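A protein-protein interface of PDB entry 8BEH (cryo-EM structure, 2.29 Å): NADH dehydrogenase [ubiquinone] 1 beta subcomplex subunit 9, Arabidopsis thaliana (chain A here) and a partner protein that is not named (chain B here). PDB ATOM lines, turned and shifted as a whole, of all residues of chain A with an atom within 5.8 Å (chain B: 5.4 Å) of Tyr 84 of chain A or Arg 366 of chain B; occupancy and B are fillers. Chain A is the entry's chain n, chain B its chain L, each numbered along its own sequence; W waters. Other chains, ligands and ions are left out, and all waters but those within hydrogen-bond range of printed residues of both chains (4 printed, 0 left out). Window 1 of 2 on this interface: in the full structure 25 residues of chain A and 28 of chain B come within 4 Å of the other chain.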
ATOM      1  N   LEU A  32     -10.879  -0.996  13.084  1.00  0.00           N
ATOM      2  CA  LEU A  32     -10.395  -2.360  12.831  1.00  0.00           C
ATOM      3  C   LEU A  32     -11.520  -3.286  12.358  1.00  0.00           C
ATOM      4  O   LEU A  32     -11.220  -4.067  11.483  1.00  0.00           O
ATOM      5  CB  LEU A  32      -9.595  -2.845  14.038  1.00  0.00           C
ATOM      6  CG  LEU A  32      -8.863  -4.179  13.906  1.00  0.00           C
ATOM      7  CD1 LEU A  32      -7.938  -4.198  12.704  1.00  0.00           C
ATOM      8  CD2 LEU A  32      -8.083  -4.461  15.171  1.00  0.00           C
ATOM      9  N   ASN A  33     -12.744  -3.167  12.863  1.00  0.00           N
ATOM     10  CA  ASN A  33     -13.908  -3.951  12.385  1.00  0.00           C
ATOM     11  C   ASN A  33     -14.214  -3.694  10.906  1.00  0.00           C
ATOM     12  O   ASN A  33     -14.587  -4.622  10.237  1.00  0.00           O
ATOM     13  CB  ASN A  33     -15.159  -3.745  13.265  1.00  0.00           C
ATOM     14  CG  ASN A  33     -14.982  -4.133  14.712  1.00  0.00           C
ATOM     15  OD1 ASN A  33     -14.452  -5.189  14.999  1.00  0.00           O
ATOM     16  ND2 ASN A  33     -15.449  -3.299  15.624  1.00  0.00           N
ATOM     17  N   VAL A  36     -10.445  -4.875   8.708  1.00  0.00           N
ATOM     18  CA  VAL A  36     -10.074  -6.317   8.746  1.00  0.00           C
ATOM     19  C   VAL A  36      -8.565  -6.474   8.539  1.00  0.00           C
ATOM     20  O   VAL A  36      -7.958  -6.936   9.450  1.00  0.00           O
ATOM     21  CB  VAL A  36     -10.983  -7.221   7.848  1.00  0.00           C
ATOM     22  CG1 VAL A  36     -10.596  -8.684   7.913  1.00  0.00           C
ATOM     23  CG2 VAL A  36     -12.456  -6.998   8.121  1.00  0.00           C
ATOM     24  N   HIS A  80     -19.943  -0.216  13.388  1.00  0.00           N
ATOM     25  CA  HIS A  80     -20.032  -1.489  12.669  1.00  0.00           C
ATOM     26  C   HIS A  80     -21.146  -2.355  13.245  1.00  0.00           C
ATOM     27  O   HIS A  80     -21.185  -2.583  14.457  1.00  0.00           O
ATOM     28  CB  HIS A  80     -18.705  -2.239  12.717  1.00  0.00           C
ATOM     29  CG  HIS A  80     -18.553  -3.268  11.641  1.00  0.00           C
ATOM     30  ND1 HIS A  80     -19.402  -4.347  11.519  1.00  0.00           N
ATOM     31  CD2 HIS A  80     -17.670  -3.368  10.618  1.00  0.00           C
ATOM     32  CE1 HIS A  80     -19.038  -5.076  10.480  1.00  0.00           C
ATOM     33  NE2 HIS A  80     -17.990  -4.503   9.916  1.00  0.00           N
ATOM     34  N   ASP A  82     -21.673  -5.520  13.357  1.00  0.00           N
ATOM     35  CA  ASP A  82     -21.272  -6.794  13.952  1.00  0.00           C
ATOM     36  C   ASP A  82     -19.837  -6.678  14.451  1.00  0.00           C
ATOM     37  O   ASP A  82     -18.904  -7.205  13.832  1.00  0.00           O
ATOM     38  CB  ASP A  82     -21.450  -7.935  12.947  1.00  0.00           C
ATOM     39  CG  ASP A  82     -20.914  -9.253  13.451  1.00  0.00           C
ATOM     40  OD1 ASP A  82     -21.273  -9.656  14.577  1.00  0.00           O
ATOM     41  OD2 ASP A  82     -20.126  -9.885  12.722  1.00  0.00           O
ATOM     42  N   PRO A  83     -19.624  -5.996  15.575  1.00  0.00           N
ATOM     43  CA  PRO A  83     -18.257  -5.806  16.076  1.00  0.00           C
ATOM     44  C   PRO A  83     -17.618  -7.105  16.539  1.00  0.00           C
ATOM     45  O   PRO A  83     -18.295  -8.046  16.956  1.00  0.00           O
ATOM     46  CB  PRO A  83     -18.440  -4.840  17.252  1.00  0.00           C
ATOM     47  CG  PRO A  83     -19.843  -5.052  17.696  1.00  0.00           C
ATOM     48  CD  PRO A  83     -20.629  -5.374  16.456  1.00  0.00           C
ATOM     49  N   TYR A  84     -16.293  -7.139  16.466  1.00  0.00           N
ATOM     50  CA  TYR A  84     -15.546  -8.274  16.982  1.00  0.00           C
ATOM     51  C   TYR A  84     -15.537  -8.262  18.505  1.00  0.00           C
ATOM     52  O   TYR A  84     -15.378  -7.213  19.132  1.00  0.00           O
ATOM     53  CB  TYR A  84     -14.105  -8.259  16.466  1.00  0.00           C
ATOM     54  CG  TYR A  84     -13.247  -9.270  17.180  1.00  0.00           C
ATOM     55  CD1 TYR A  84     -13.319 -10.619  16.855  1.00  0.00           C
ATOM     56  CD2 TYR A  84     -12.408  -8.890  18.221  1.00  0.00           C
ATOM     57  CE1 TYR A  84     -12.564 -11.550  17.525  1.00  0.00           C
ATOM     58  CE2 TYR A  84     -11.651  -9.818  18.898  1.00  0.00           C
ATOM     59  CZ  TYR A  84     -11.731 -11.147  18.547  1.00  0.00           C
ATOM     60  OH  TYR A  84     -10.974 -12.073  19.214  1.00  0.00           O
ATOM     61  N   ILE A  85     -15.695  -9.437  19.101  1.00  0.00           N
ATOM     62  CA  ILE A  85     -15.589  -9.602  20.546  1.00  0.00           C
ATOM     63  C   ILE A  85     -14.714 -10.812  20.832  1.00  0.00           C
ATOM     64  O   ILE A  85     -14.876 -11.864  20.207  1.00  0.00           O
ATOM     65  CB  ILE A  85     -16.970  -9.760  21.222  1.00  0.00           C
ATOM     66  CG1 ILE A  85     -17.884  -8.582  20.892  1.00  0.00           C
ATOM     67  CG2 ILE A  85     -16.822  -9.911  22.733  1.00  0.00           C
ATOM     68  CD1 ILE A  85     -19.302  -8.977  20.579  1.00  0.00           C
ATOM     69  N   VAL A  86     -13.793 -10.660  21.777  1.00  0.00           N
ATOM     70  CA  VAL A  86     -13.025 -11.809  22.271  1.00  0.00           C
ATOM     71  C   VAL A  86     -13.994 -12.873  22.777  1.00  0.00           C
ATOM     72  O   VAL A  86     -14.961 -12.538  23.487  1.00  0.00           O
ATOM     73  CB  VAL A  86     -12.054 -11.365  23.381  1.00  0.00           C
ATOM     74  CG1 VAL A  86     -11.198 -12.521  23.860  1.00  0.00           C
ATOM     75  CG2 VAL A  86     -11.175 -10.226  22.886  1.00  0.00           C
ATOM     76  N   PRO A  87     -13.798 -14.151  22.435  1.00  0.00           N
ATOM     77  CA  PRO A  87     -14.850 -15.153  22.693  1.00  0.00           C
ATOM     78  C   PRO A  87     -15.277 -15.281  24.148  1.00  0.00           C
ATOM     79  O   PRO A  87     -16.449 -15.574  24.405  1.00  0.00           O
ATOM     80  CB  PRO A  87     -14.220 -16.451  22.170  1.00  0.00           C
ATOM     81  CG  PRO A  87     -13.234 -16.009  21.163  1.00  0.00           C
ATOM     82  CD  PRO A  87     -12.684 -14.708  21.648  1.00  0.00           C
ATOM     83  N   ASN B 305     -19.344 -12.755   9.434  1.00  0.00           N
ATOM     84  CA  ASN B 305     -17.973 -12.834   9.910  1.00  0.00           C
ATOM     85  C   ASN B 305     -17.676 -14.097  10.704  1.00  0.00           C
ATOM     86  O   ASN B 305     -16.502 -14.402  10.929  1.00  0.00           O
ATOM     87  CB  ASN B 305     -17.645 -11.611  10.778  1.00  0.00           C
ATOM     88  CG  ASN B 305     -17.676 -10.318   9.990  1.00  0.00           C
ATOM     89  OD1 ASN B 305     -18.451  -9.416  10.294  1.00  0.00           O
ATOM     90  ND2 ASN B 305     -16.850 -10.232   8.962  1.00  0.00           N
ATOM     91  N   GLU B 362     -11.647 -19.341  18.594  1.00  0.00           N
ATOM     92  CA  GLU B 362     -11.907 -18.158  17.790  1.00  0.00           C
ATOM     93  C   GLU B 362     -12.759 -18.558  16.591  1.00  0.00           C
ATOM     94  O   GLU B 362     -12.443 -19.520  15.886  1.00  0.00           O
ATOM     95  CB  GLU B 362     -10.600 -17.510  17.333  1.00  0.00           C
ATOM     96  CG  GLU B 362     -10.787 -16.268  16.480  1.00  0.00           C
ATOM     97  CD  GLU B 362     -11.495 -15.148  17.224  1.00  0.00           C
ATOM     98  OE1 GLU B 362     -10.931 -14.631  18.211  1.00  0.00           O
ATOM     99  OE2 GLU B 362     -12.618 -14.785  16.825  1.00  0.00           O
ATOM    100  N   ASP B 364     -14.282 -15.818  14.571  1.00  0.00           N
ATOM    101  CA  ASP B 364     -14.370 -14.660  13.695  1.00  0.00           C
ATOM    102  C   ASP B 364     -13.278 -14.736  12.637  1.00  0.00           C
ATOM    103  O   ASP B 364     -12.089 -14.803  12.967  1.00  0.00           O
ATOM    104  CB  ASP B 364     -14.255 -13.368  14.502  1.00  0.00           C
ATOM    105  CG  ASP B 364     -15.015 -12.224  13.879  1.00  0.00           C
ATOM    106  OD1 ASP B 364     -14.488 -11.609  12.933  1.00  0.00           O
ATOM    107  OD2 ASP B 364     -16.139 -11.937  14.330  1.00  0.00           O
ATOM    108  N   MET B 365     -13.683 -14.714  11.366  1.00  0.00           N
ATOM    109  CA  MET B 365     -12.728 -14.815  10.269  1.00  0.00           C
ATOM    110  C   MET B 365     -11.820 -13.598  10.176  1.00  0.00           C
ATOM    111  O   MET B 365     -10.741 -13.693   9.585  1.00  0.00           O
ATOM    112  CB  MET B 365     -13.468 -15.026   8.944  1.00  0.00           C
ATOM    113  CG  MET B 365     -14.117 -16.392   8.819  1.00  0.00           C
ATOM    114  SD  MET B 365     -14.966 -16.680   7.255  1.00  0.00           S
ATOM    115  CE  MET B 365     -16.157 -15.346   7.234  1.00  0.00           C
ATOM    116  N   ARG B 366     -12.223 -12.464  10.751  1.00  0.00           N
ATOM    117  CA  ARG B 366     -11.376 -11.279  10.751  1.00  0.00           C
ATOM    118  C   ARG B 366     -10.164 -11.417  11.664  1.00  0.00           C
ATOM    119  O   ARG B 366      -9.277 -10.562  11.612  1.00  0.00           O
ATOM    120  CB  ARG B 366     -12.184 -10.048  11.158  1.00  0.00           C
ATOM    121  CG  ARG B 366     -13.471  -9.830  10.384  1.00  0.00           C
ATOM    122  CD  ARG B 366     -14.227  -8.664  10.985  1.00  0.00           C
ATOM    123  NE  ARG B 366     -15.016  -9.078  12.138  1.00  0.00           N
ATOM    124  CZ  ARG B 366     -16.185  -8.556  12.479  1.00  0.00           C
ATOM    125  NH1 ARG B 366     -16.695  -7.522  11.832  1.00  0.00           N
ATOM    126  NH2 ARG B 366     -16.850  -9.072  13.507  1.00  0.00           N
ATOM    127  N   LYS B 367     -10.048 -12.457  12.442  1.00  0.00           N
ATOM    128  CA  LYS B 367      -8.927 -12.677  13.387  1.00  0.00           C
ATOM    129  C   LYS B 367      -8.269 -14.005  13.016  1.00  0.00           C
ATOM    130  O   LYS B 367      -7.821 -14.684  13.879  1.00  0.00           O
ATOM    131  CB  LYS B 367      -9.415 -12.521  14.857  1.00  0.00           C
ATOM    132  CG  LYS B 367     -10.049 -11.197  15.227  1.00  0.00           C
ATOM    133  CD  LYS B 367      -9.087 -10.058  15.261  1.00  0.00           C
ATOM    134  CE  LYS B 367      -9.809  -8.735  15.359  1.00  0.00           C
ATOM    135  NZ  LYS B 367      -8.953  -7.612  14.939  1.00  0.00           N
ATOM    136  N   MET B 368      -8.196 -14.307  11.738  1.00  0.00           N
ATOM    137  CA  MET B 368      -7.668 -15.566  11.234  1.00  0.00           C
ATOM    138  C   MET B 368      -6.717 -15.215  10.095  1.00  0.00           C
ATOM    139  O   MET B 368      -6.229 -14.085   9.994  1.00  0.00           O
ATOM    140  CB  MET B 368      -8.813 -16.501  10.812  1.00  0.00           C
ATOM    141  CG  MET B 368      -9.380 -17.356  11.939  1.00  0.00           C
ATOM    142  SD  MET B 368     -10.890 -18.226  11.472  1.00  0.00           S
ATOM    143  CE  MET B 368     -11.862 -18.098  12.974  1.00  0.00           C
ATOM    144  N   ASN B 447      -4.395 -12.083  10.331  1.00  0.00           N
ATOM    145  CA  ASN B 447      -5.009 -11.050  11.150  1.00  0.00           C
ATOM    146  C   ASN B 447      -5.288 -11.551  12.560  1.00  0.00           C
ATOM    147  O   ASN B 447      -6.091 -10.956  13.284  1.00  0.00           O
ATOM    148  CB  ASN B 447      -6.303 -10.557  10.505  1.00  0.00           C
ATOM    149  CG  ASN B 447      -6.061  -9.718   9.276  1.00  0.00           C
ATOM    150  OD1 ASN B 447      -5.229  -8.812   9.277  1.00  0.00           O
ATOM    151  ND2 ASN B 447      -6.799 -10.010   8.214  1.00  0.00           N
ATOM    152  N   SER B 448      -4.651 -12.644  12.956  1.00  0.00           N
ATOM    153  CA  SER B 448      -4.951 -13.300  14.215  1.00  0.00           C
ATOM    154  C   SER B 448      -4.106 -12.731  15.351  1.00  0.00           C
ATOM    155  O   SER B 448      -3.237 -11.880  15.161  1.00  0.00           O
ATOM    156  CB  SER B 448      -4.727 -14.807  14.094  1.00  0.00           C
ATOM    157  OG  SER B 448      -3.364 -15.102  13.888  1.00  0.00           O
ATOM    158  N   PHE B 449      -4.311 -13.282  16.528  1.00  0.00           N
ATOM    159  CA  PHE B 449      -3.582 -12.902  17.744  1.00  0.00           C
ATOM    160  C   PHE B 449      -2.385 -13.855  17.844  1.00  0.00           C
ATOM    161  O   PHE B 449      -2.548 -15.019  17.519  1.00  0.00           O
ATOM    162  CB  PHE B 449      -4.590 -13.011  18.903  1.00  0.00           C
ATOM    163  CG  PHE B 449      -5.670 -11.961  18.963  1.00  0.00           C
ATOM    164  CD1 PHE B 449      -6.929 -12.200  18.438  1.00  0.00           C
ATOM    165  CD2 PHE B 449      -5.454 -10.751  19.600  1.00  0.00           C
ATOM    166  CE1 PHE B 449      -7.934 -11.250  18.518  1.00  0.00           C
ATOM    167  CE2 PHE B 449      -6.457  -9.797  19.678  1.00  0.00           C
ATOM    168  CZ  PHE B 449      -7.697 -10.048  19.140  1.00  0.00           C
HETATM  169  O   HOH W   1      -8.898  -7.757  11.904  1.00  0.00           O
HETATM  170  O   HOH W   2     -16.303 -11.741  17.186  1.00  0.00           O
HETATM  171  O   HOH W   3     -14.466 -13.711  18.495  1.00  0.00           O
HETATM  172  O   HOH W   4     -11.792  -5.720  14.940  1.00  0.00           O
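NH2 of Arg 366 of chain B is in salt-bridge range of OD2 of Asp 82 of chain A (3.5 Å). The side-chain amide oxygen (OD1) of Asn 447 of chain B lies close to the backbone carbonyl oxygen (O) of Val 36 of chain A, 3.3 Å away. OD1 of Asn 305 of chain B sits close to OD2 of Asp 82 of chain A (3.0 Å). The side-chain carboxylate (OE1) of Glu 362 of chain B is in hydrogen-bond range of the side-chain hydroxyl (OH) of Tyr 84 of chain A, at 2.7 Å.
NZ of Lys 367 of chain B touches CD2 of Leu 32 of chain A, at 3.3 Å. O of Asn 33 of chain A touches NH1 of Arg 366 of chain B, at 3.9 Å. Val 36 of chain A touches Arg 366 of chain B. CE1 of His 80 of chain A touches NH1 of Arg 366 of chain B (3.6 Å). Pro 83 of chain A touches Arg 366 of chain B. CB of Asp 364 of chain B touches CD1 of Tyr 84 of chain A (3.7 Å). Arg 366 of chain B touches Tyr 84 of chain A. CE1 of Tyr 84 of chain A touches CG of Lys 367 of chain B, 3.4 Å away. Phe 449 of chain B touches Tyr 84 of chain A. Pro 87 of chain A touches Glu 362 of chain B.
Of the 10 printed residues of chain B, 7 touch a printed residue of chain A. Hydrophobic or aromatic side chains of chain B that line the printed part of chain A: Phe 449. Hydrophobic or aromatic side chains of chain A that line the printed part of chain B: Leu 32, Val 36, His 80, Tyr 84 and Pro 87. Among the printed residues, 14 pairs touch across the chains. Among the printed residues, Asp or Glu carboxylates within 4 Å of a Lys or Arg side-chain nitrogen of the other chain: Asp 82 of chain A with Arg 366 of chain B (3.5 Å).
Water W3 bridges the backbone carbonyl oxygen of Ile 85 of chain A (2.6 Å) and the side-chain carboxylate of Glu 362 of chain B (2.7 Å). Water W4 lies within hydrogen-bond range of OD1 of Asn 33 of chain A and NZ of Lys 367 of chain B. Water W1 lies within hydrogen-bond range of the backbone carbonyl oxygen of Val 36 of chain A, the backbone carbonyl oxygen of Arg 366 of chain B and the side-chain amino group of Lys 367 of chain B. Water W2 lies within hydrogen-bond range of OD2 of Asp 364 of chain B and N of Ile 85 of chain A.
Printed residues of chain B within 4 Å of Asn 33 of chain A: Arg 366. Printed residues of chain B within 4 Å of Tyr 84 of chain A: Glu 362 (2.7 Å), Asp 364 (3.7 Å), Arg 366 (3.6 Å), Lys 367 (3.4 Å) and Phe 449 (3.2 Å). Met 365 of chain B touches none of the printed residues of chain A. Of chain A, only Asn 33 (3.9 Å), Val 36 (3.8 Å), His 80 (3.6 Å), Asp 82 (2.8 Å), Pro 83 (3.7 Å) and Tyr 84 (3.6 Å) come within 4 Å of Arg 366 of chain B. Of the printed residues of chain A, Lys 367 of chain B touches Leu 32 (3.3 Å) and Tyr 84 (3.4 Å). The nearest printed residue of chain B that does not touch Tyr 84 of chain A is Met 365 of chain B (6.9 Å). The nearest printed residue of chain B that does not touch Asn 33 of chain A is Lys 367 of chain B (5.9 Å).
The side-chain carboxylate (OE2) of Glu 362 of chain B lies within hydrogen-bond range of the backbone NH (N) of Asp 364 of chain B, 3.0 Å away. O of Asn 305 of chain B sits at hydrogen-bond distance from N of Met 365 of chain B (2.9 Å). The backbone NH (N) of Asp 82 of chain A sits at hydrogen-bond distance from a ring nitrogen (ND1) of His 80 of chain A (3.1 Å). The backbone carbonyl oxygen (O) of Asn 33 of chain A lies close to a ring nitrogen (NE2) of His 80 of chain A (3.4 Å). N of Tyr 84 of chain A lies within hydrogen-bond range of OD1 of Asn 33 of chain A. O of Met 368 of chain B lies within hydrogen-bond range of N of Asn 447 of chain B, 2.7 Å away.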
